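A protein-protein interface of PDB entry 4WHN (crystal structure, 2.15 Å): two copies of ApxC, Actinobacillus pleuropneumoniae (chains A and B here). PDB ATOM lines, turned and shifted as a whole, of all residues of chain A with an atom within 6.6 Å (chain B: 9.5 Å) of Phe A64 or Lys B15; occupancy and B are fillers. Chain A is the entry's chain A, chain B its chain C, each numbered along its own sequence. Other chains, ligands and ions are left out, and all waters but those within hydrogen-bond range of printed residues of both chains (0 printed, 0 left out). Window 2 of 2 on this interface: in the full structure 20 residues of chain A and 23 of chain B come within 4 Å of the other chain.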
ATOM      1  N   GLU A  20      -8.750   9.759  11.872  1.00  0.00           N
ATOM      2  CA  GLU A  20      -9.822  10.241  11.064  1.00  0.00           C
ATOM      3  C   GLU A  20      -9.336  11.403  10.240  1.00  0.00           C
ATOM      4  O   GLU A  20      -9.630  11.510   9.032  1.00  0.00           O
ATOM      5  CB  GLU A  20     -11.007  10.714  11.896  1.00  0.00           C
ATOM      6  CG  GLU A  20     -12.019  11.297  10.953  1.00  0.00           C
ATOM      7  CD  GLU A  20     -13.334  11.673  11.541  1.00  0.00           C
ATOM      8  OE1 GLU A  20     -13.710  11.117  12.596  1.00  0.00           O
ATOM      9  OE2 GLU A  20     -13.999  12.520  10.893  1.00  0.00           O
ATOM     10  N   GLU A  24      -9.016  11.797   6.116  1.00  0.00           N
ATOM     11  CA  GLU A  24      -9.630  12.867   5.366  1.00  0.00           C
ATOM     12  C   GLU A  24      -8.594  13.535   4.511  1.00  0.00           C
ATOM     13  O   GLU A  24      -8.802  13.756   3.313  1.00  0.00           O
ATOM     14  CB  GLU A  24     -10.293  13.853   6.335  1.00  0.00           C
ATOM     15  CG  GLU A  24     -11.537  13.283   6.990  1.00  0.00           C
ATOM     16  CD  GLU A  24     -12.270  14.348   7.815  1.00  0.00           C
ATOM     17  OE1 GLU A  24     -12.156  14.312   9.046  1.00  0.00           O
ATOM     18  OE2 GLU A  24     -12.906  15.237   7.206  1.00  0.00           O
ATOM     19  N   TRP A  27      -7.525  11.355   1.608  1.00  0.00           N
ATOM     20  CA  TRP A  27      -8.584  11.362   0.566  1.00  0.00           C
ATOM     21  C   TRP A  27      -8.465  12.591  -0.261  1.00  0.00           C
ATOM     22  O   TRP A  27      -8.496  12.548  -1.495  1.00  0.00           O
ATOM     23  CB  TRP A  27      -9.936  11.274   1.221  1.00  0.00           C
ATOM     24  CG  TRP A  27     -11.019  11.173   0.239  1.00  0.00           C
ATOM     25  CD1 TRP A  27     -11.320  10.100  -0.510  1.00  0.00           C
ATOM     26  CD2 TRP A  27     -11.951  12.192  -0.122  1.00  0.00           C
ATOM     27  NE1 TRP A  27     -12.369  10.376  -1.323  1.00  0.00           N
ATOM     28  CE2 TRP A  27     -12.781  11.658  -1.100  1.00  0.00           C
ATOM     29  CE3 TRP A  27     -12.170  13.497   0.309  1.00  0.00           C
ATOM     30  CZ2 TRP A  27     -13.837  12.364  -1.664  1.00  0.00           C
ATOM     31  CZ3 TRP A  27     -13.240  14.219  -0.260  1.00  0.00           C
ATOM     32  CH2 TRP A  27     -14.037  13.645  -1.254  1.00  0.00           C
ATOM     33  N   LEU A  59     -11.241  22.334   6.164  1.00  0.00           N
ATOM     34  CA  LEU A  59     -12.594  22.805   5.864  1.00  0.00           C
ATOM     35  C   LEU A  59     -13.394  21.663   5.321  1.00  0.00           C
ATOM     36  O   LEU A  59     -12.892  20.841   4.539  1.00  0.00           O
ATOM     37  CB  LEU A  59     -12.596  23.896   4.792  1.00  0.00           C
ATOM     38  CG  LEU A  59     -11.878  25.174   5.087  1.00  0.00           C
ATOM     39  CD1 LEU A  59     -12.027  26.126   3.923  1.00  0.00           C
ATOM     40  CD2 LEU A  59     -12.410  25.800   6.355  1.00  0.00           C
ATOM     41  N   LYS A  60     -14.655  21.647   5.715  1.00  0.00           N
ATOM     42  CA  LYS A  60     -15.571  20.597   5.353  1.00  0.00           C
ATOM     43  C   LYS A  60     -16.813  21.210   4.751  1.00  0.00           C
ATOM     44  O   LYS A  60     -17.133  22.356   4.967  1.00  0.00           O
ATOM     45  CB  LYS A  60     -15.955  19.817   6.607  1.00  0.00           C
ATOM     46  CG  LYS A  60     -14.807  19.051   7.220  1.00  0.00           C
ATOM     47  CD  LYS A  60     -15.373  17.944   8.109  1.00  0.00           C
ATOM     48  CE  LYS A  60     -14.510  17.506   9.279  1.00  0.00           C
ATOM     49  NZ  LYS A  60     -15.208  16.392   9.996  1.00  0.00           N
ATOM     50  N   ARG A  61     -17.555  20.457   3.990  1.00  0.00           N
ATOM     51  CA  ARG A  61     -18.842  21.012   3.614  1.00  0.00           C
ATOM     52  C   ARG A  61     -20.052  20.304   4.226  1.00  0.00           C
ATOM     53  O   ARG A  61     -20.523  20.662   5.320  1.00  0.00           O
ATOM     54  CB  ARG A  61     -18.906  21.287   2.106  1.00  0.00           C
ATOM     55  CG  ARG A  61     -20.246  21.854   1.753  1.00  0.00           C
ATOM     56  CD  ARG A  61     -20.322  22.342   0.378  1.00  0.00           C
ATOM     57  NE  ARG A  61     -19.373  23.412   0.159  1.00  0.00           N
ATOM     58  CZ  ARG A  61     -18.414  23.365  -0.751  1.00  0.00           C
ATOM     59  NH1 ARG A  61     -18.262  22.293  -1.524  1.00  0.00           N
ATOM     60  NH2 ARG A  61     -17.598  24.394  -0.885  1.00  0.00           N
ATOM     61  N   ASP A  62     -20.554  19.323   3.507  1.00  0.00           N
ATOM     62  CA  ASP A  62     -21.629  18.463   3.973  1.00  0.00           C
ATOM     63  C   ASP A  62     -21.002  17.250   4.675  1.00  0.00           C
ATOM     64  O   ASP A  62     -21.193  16.130   4.211  1.00  0.00           O
ATOM     65  CB  ASP A  62     -22.438  18.058   2.737  1.00  0.00           C
ATOM     66  CG  ASP A  62     -23.249  19.252   2.108  1.00  0.00           C
ATOM     67  OD1 ASP A  62     -23.834  20.065   2.861  1.00  0.00           O
ATOM     68  OD2 ASP A  62     -23.306  19.377   0.854  1.00  0.00           O
ATOM     69  N   GLY A  63     -20.251  17.465   5.773  1.00  0.00           N
ATOM     70  CA  GLY A  63     -19.506  16.381   6.457  1.00  0.00           C
ATOM     71  C   GLY A  63     -18.365  15.747   5.666  1.00  0.00           C
ATOM     72  O   GLY A  63     -17.764  14.766   6.122  1.00  0.00           O
ATOM     73  N   PHE A  64     -18.067  16.268   4.477  1.00  0.00           N
ATOM     74  CA  PHE A  64     -16.917  15.800   3.715  1.00  0.00           C
ATOM     75  C   PHE A  64     -15.848  16.884   3.761  1.00  0.00           C
ATOM     76  O   PHE A  64     -16.163  18.057   3.674  1.00  0.00           O
ATOM     77  CB  PHE A  64     -17.297  15.449   2.272  1.00  0.00           C
ATOM     78  CG  PHE A  64     -17.879  14.082   2.110  1.00  0.00           C
ATOM     79  CD1 PHE A  64     -19.188  13.821   2.488  1.00  0.00           C
ATOM     80  CD2 PHE A  64     -17.127  13.047   1.546  1.00  0.00           C
ATOM     81  CE1 PHE A  64     -19.737  12.558   2.318  1.00  0.00           C
ATOM     82  CE2 PHE A  64     -17.668  11.780   1.379  1.00  0.00           C
ATOM     83  CZ  PHE A  64     -18.978  11.538   1.763  1.00  0.00           C
ATOM     84  N   PRO A  65     -14.577  16.487   3.899  1.00  0.00           N
ATOM     85  CA  PRO A  65     -13.550  17.474   3.722  1.00  0.00           C
ATOM     86  C   PRO A  65     -13.542  18.058   2.330  1.00  0.00           C
ATOM     87  O   PRO A  65     -13.717  17.342   1.349  1.00  0.00           O
ATOM     88  CB  PRO A  65     -12.244  16.657   3.909  1.00  0.00           C
ATOM     89  CG  PRO A  65     -12.591  15.305   3.404  1.00  0.00           C
ATOM     90  CD  PRO A  65     -14.016  15.116   3.868  1.00  0.00           C
ATOM     91  N   ILE A  66     -13.203  19.332   2.223  1.00  0.00           N
ATOM     92  CA  ILE A  66     -12.955  19.938   0.897  1.00  0.00           C
ATOM     93  C   ILE A  66     -11.603  20.612   0.745  1.00  0.00           C
ATOM     94  O   ILE A  66     -11.167  20.881  -0.382  1.00  0.00           O
ATOM     95  CB  ILE A  66     -14.061  20.967   0.566  1.00  0.00           C
ATOM     96  CG1 ILE A  66     -14.158  22.018   1.657  1.00  0.00           C
ATOM     97  CG2 ILE A  66     -15.411  20.236   0.453  1.00  0.00           C
ATOM     98  CD1 ILE A  66     -14.974  23.227   1.260  1.00  0.00           C
ATOM     99  N   ALA A  67     -10.974  20.993   1.855  1.00  0.00           N
ATOM    100  CA  ALA A  67      -9.720  21.734   1.751  1.00  0.00           C
ATOM    101  C   ALA A  67      -8.911  21.582   3.011  1.00  0.00           C
ATOM    102  O   ALA A  67      -9.476  21.405   4.113  1.00  0.00           O
ATOM    103  CB  ALA A  67      -9.972  23.210   1.495  1.00  0.00           C
ATOM    104  N   LYS B  15     -19.208   6.220   7.957  1.00  0.00           N
ATOM    105  CA  LYS B  15     -18.468   7.184   7.049  1.00  0.00           C
ATOM    106  C   LYS B  15     -17.406   8.070   7.750  1.00  0.00           C
ATOM    107  O   LYS B  15     -16.336   8.375   7.176  1.00  0.00           O
ATOM    108  CB  LYS B  15     -19.464   8.052   6.248  1.00  0.00           C
ATOM    109  CG  LYS B  15     -18.897   9.218   5.438  1.00  0.00           C
ATOM    110  CD  LYS B  15     -17.789   8.861   4.458  1.00  0.00           C
ATOM    111  CE  LYS B  15     -18.377   8.206   3.208  1.00  0.00           C
ATOM    112  NZ  LYS B  15     -17.362   7.480   2.406  1.00  0.00           N
ATOM    113  N   ILE B  16     -17.685   8.455   8.989  1.00  0.00           N
ATOM    114  CA  ILE B  16     -16.635   9.013   9.844  1.00  0.00           C
ATOM    115  C   ILE B  16     -15.705   7.837  10.196  1.00  0.00           C
ATOM    116  O   ILE B  16     -14.475   7.954  10.196  1.00  0.00           O
ATOM    117  CB  ILE B  16     -17.230   9.796  11.071  1.00  0.00           C
ATOM    118  CG1 ILE B  16     -17.094  11.321  10.856  1.00  0.00           C
ATOM    119  CG2 ILE B  16     -16.570   9.395  12.397  1.00  0.00           C
ATOM    120  CD1 ILE B  16     -17.509  11.853   9.482  1.00  0.00           C
ATOM    121  N   ASN B  17     -16.327   6.707  10.489  1.00  0.00           N
ATOM    122  CA  ASN B  17     -15.646   5.435  10.579  1.00  0.00           C
ATOM    123  C   ASN B  17     -14.776   5.173   9.355  1.00  0.00           C
ATOM    124  O   ASN B  17     -13.655   4.720   9.494  1.00  0.00           O
ATOM    125  CB  ASN B  17     -16.683   4.336  10.720  1.00  0.00           C
ATOM    126  CG  ASN B  17     -16.063   2.982  10.938  1.00  0.00           C
ATOM    127  OD1 ASN B  17     -16.157   2.098  10.088  1.00  0.00           O
ATOM    128  ND2 ASN B  17     -15.452   2.799  12.093  1.00  0.00           N
ATOM    129  N   GLY B  18     -15.319   5.430   8.171  1.00  0.00           N
ATOM    130  CA  GLY B  18     -14.592   5.229   6.916  1.00  0.00           C
ATOM    131  C   GLY B  18     -13.243   5.937   6.805  1.00  0.00           C
ATOM    132  O   GLY B  18     -12.205   5.336   6.467  1.00  0.00           O
ATOM    133  N   PHE B  19     -13.261   7.215   7.116  1.00  0.00           N
ATOM    134  CA  PHE B  19     -12.060   8.013   7.098  1.00  0.00           C
ATOM    135  C   PHE B  19     -11.092   7.569   8.167  1.00  0.00           C
ATOM    136  O   PHE B  19      -9.891   7.593   7.984  1.00  0.00           O
ATOM    137  CB  PHE B  19     -12.430   9.484   7.291  1.00  0.00           C
ATOM    138  CG  PHE B  19     -12.941  10.143   6.053  1.00  0.00           C
ATOM    139  CD1 PHE B  19     -12.167  10.186   4.892  1.00  0.00           C
ATOM    140  CD2 PHE B  19     -14.177  10.793   6.046  1.00  0.00           C
ATOM    141  CE1 PHE B  19     -12.613  10.833   3.750  1.00  0.00           C
ATOM    142  CE2 PHE B  19     -14.630  11.429   4.892  1.00  0.00           C
ATOM    143  CZ  PHE B  19     -13.823  11.483   3.761  1.00  0.00           C
ATOM    144  N   GLU B  20     -11.618   7.141   9.287  1.00  0.00           N
ATOM    145  CA  GLU B  20     -10.775   6.714  10.367  1.00  0.00           C
ATOM    146  C   GLU B  20      -9.999   5.461   9.938  1.00  0.00           C
ATOM    147  O   GLU B  20      -8.776   5.320  10.161  1.00  0.00           O
ATOM    148  CB  GLU B  20     -11.656   6.470  11.580  1.00  0.00           C
ATOM    149  CG  GLU B  20     -10.906   6.333  12.904  1.00  0.00           C
ATOM    150  CD  GLU B  20     -10.324   4.971  13.077  1.00  0.00           C
ATOM    151  OE1 GLU B  20     -10.886   4.022  12.507  1.00  0.00           O
ATOM    152  OE2 GLU B  20      -9.326   4.857  13.805  1.00  0.00           O
ATOM    153  N   VAL B  21     -10.707   4.540   9.299  1.00  0.00           N
ATOM    154  CA  VAL B  21     -10.052   3.321   8.843  1.00  0.00           C
ATOM    155  C   VAL B  21      -9.045   3.668   7.770  1.00  0.00           C
ATOM    156  O   VAL B  21      -7.915   3.119   7.763  1.00  0.00           O
ATOM    157  CB  VAL B  21     -11.091   2.316   8.295  1.00  0.00           C
ATOM    158  CG1 VAL B  21     -10.421   1.192   7.511  1.00  0.00           C
ATOM    159  CG2 VAL B  21     -11.935   1.759   9.445  1.00  0.00           C
ATOM    160  N   LEU B  22      -9.443   4.545   6.842  1.00  0.00           N
ATOM    161  CA  LEU B  22      -8.539   4.929   5.786  1.00  0.00           C
ATOM    162  C   LEU B  22      -7.230   5.504   6.379  1.00  0.00           C
ATOM    163  O   LEU B  22      -6.131   5.274   5.848  1.00  0.00           O
ATOM    164  CB  LEU B  22      -9.195   5.955   4.882  1.00  0.00           C
ATOM    165  CG  LEU B  22      -8.341   6.460   3.710  1.00  0.00           C
ATOM    166  CD1 LEU B  22      -7.975   5.363   2.727  1.00  0.00           C
ATOM    167  CD2 LEU B  22      -9.044   7.568   2.986  1.00  0.00           C
ATOM    168  N   GLY B  23      -7.356   6.277   7.462  1.00  0.00           N
ATOM    169  CA  GLY B  23      -6.207   6.916   8.121  1.00  0.00           C
ATOM    170  C   GLY B  23      -5.309   5.873   8.732  1.00  0.00           C
ATOM    171  O   GLY B  23      -4.080   5.895   8.576  1.00  0.00           O
ATOM    172  N   LEU B  48     -10.215   2.340  -0.759  1.00  0.00           N
ATOM    173  CA  LEU B  48     -11.623   2.850  -0.632  1.00  0.00           C
ATOM    174  C   LEU B  48     -12.644   1.773  -0.927  1.00  0.00           C
ATOM    175  O   LEU B  48     -13.552   1.567  -0.142  1.00  0.00           O
ATOM    176  CB  LEU B  48     -11.861   4.060  -1.508  1.00  0.00           C
ATOM    177  CG  LEU B  48     -11.068   5.305  -1.031  1.00  0.00           C
ATOM    178  CD1 LEU B  48     -11.254   6.448  -2.022  1.00  0.00           C
ATOM    179  CD2 LEU B  48     -11.521   5.708   0.362  1.00  0.00           C
ATOM    180  N   PRO B  49     -12.450   1.006  -1.990  1.00  0.00           N
ATOM    181  CA  PRO B  49     -13.462  -0.041  -2.220  1.00  0.00           C
ATOM    182  C   PRO B  49     -13.452  -1.134  -1.186  1.00  0.00           C
ATOM    183  O   PRO B  49     -14.487  -1.790  -0.966  1.00  0.00           O
ATOM    184  CB  PRO B  49     -13.079  -0.589  -3.622  1.00  0.00           C
ATOM    185  CG  PRO B  49     -12.307   0.557  -4.256  1.00  0.00           C
ATOM    186  CD  PRO B  49     -11.496   1.082  -3.119  1.00  0.00           C
ATOM    187  N   ILE B  51     -12.902  -0.745   1.974  1.00  0.00           N
ATOM    188  CA  ILE B  51     -13.669  -0.219   3.093  1.00  0.00           C
ATOM    189  C   ILE B  51     -15.172  -0.181   2.790  1.00  0.00           C
ATOM    190  O   ILE B  51     -15.981  -0.523   3.619  1.00  0.00           O
ATOM    191  CB  ILE B  51     -13.189   1.198   3.470  1.00  0.00           C
ATOM    192  CG1 ILE B  51     -11.745   1.166   3.979  1.00  0.00           C
ATOM    193  CG2 ILE B  51     -14.108   1.827   4.509  1.00  0.00           C
ATOM    194  CD1 ILE B  51     -11.143   2.555   4.181  1.00  0.00           C
ATOM    195  N   GLU B  52     -15.513   0.250   1.580  1.00  0.00           N
ATOM    196  CA  GLU B  52     -16.901   0.421   1.173  1.00  0.00           C
ATOM    197  C   GLU B  52     -17.635  -0.906   1.141  1.00  0.00           C
ATOM    198  O   GLU B  52     -18.788  -0.976   1.518  1.00  0.00           O
ATOM    199  CB  GLU B  52     -16.960   1.057  -0.224  1.00  0.00           C
ATOM    200  CG  GLU B  52     -18.081   2.075  -0.434  1.00  0.00           C
ATOM    201  CD  GLU B  52     -17.880   3.377   0.325  1.00  0.00           C
ATOM    202  OE1 GLU B  52     -17.101   4.242  -0.144  1.00  0.00           O
ATOM    203  OE2 GLU B  52     -18.544   3.559   1.350  1.00  0.00           O
ATOM    204  N   ASN B  54     -16.614  -3.547   2.795  1.00  0.00           N
ATOM    205  CA  ASN B  54     -16.227  -4.240   4.011  1.00  0.00           C
ATOM    206  C   ASN B  54     -15.424  -5.525   3.768  1.00  0.00           C
ATOM    207  O   ASN B  54     -15.392  -6.410   4.603  1.00  0.00           O
ATOM    208  CB  ASN B  54     -17.411  -4.406   4.966  1.00  0.00           C
ATOM    209  CG  ASN B  54     -17.908  -3.056   5.543  1.00  0.00           C
ATOM    210  OD1 ASN B  54     -17.123  -2.263   6.059  1.00  0.00           O
ATOM    211  ND2 ASN B  54     -19.213  -2.784   5.430  1.00  0.00           N
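The side-chain carboxylate (OE2) of Glu A24 is in salt-bridge range of the side-chain amino group (NZ) of Lys A60, at 3.8 Å.
Among the printed residues, merely in contact across the chains: Glu A20 with Ile B16, Glu A20 with Phe B19, Glu A20 with Glu B20, Glu A24 with Phe B19, Trp A27 with Phe B19, Trp A27 with Leu B48, Phe A64 with Lys B15 and Pro A65 with Phe B19.
Printed residues of chain B within 4 Å of Glu A20: Ile B16, Phe B19 and Glu B20. Printed residues of chain B within 4 Å of Glu A24: Phe B19 (3.6 Å). No residue of chain B comes within 4 Å of Gly A63. Of the printed residues of chain A, Lys B15 touches Phe A64. Leu B22 touches none of the printed residues of chain A. The nearest residue of chain A that does not touch Lys B15 is Gly A63 (5.7 Å). The nearest printed residue of chain B that does not touch Trp A27 is Leu B22 (4.2 Å).
Of the 14 printed residues of chain B, 5 touch a printed residue of chain A. Hydrophobic or aromatic side chains of chain B within 4 Å of the printed part of chain A: Ile B16, Phe B19 and Leu B48. Along chain A the printed residues that touch a printed residue of chain B span positions 20 to 65. Among the printed residues, no Asp or Glu carboxylate lies within 4 Å of a Lys or Arg side-chain nitrogen of the other chain.
Glu B20 touches its own counterpart, Glu A20.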
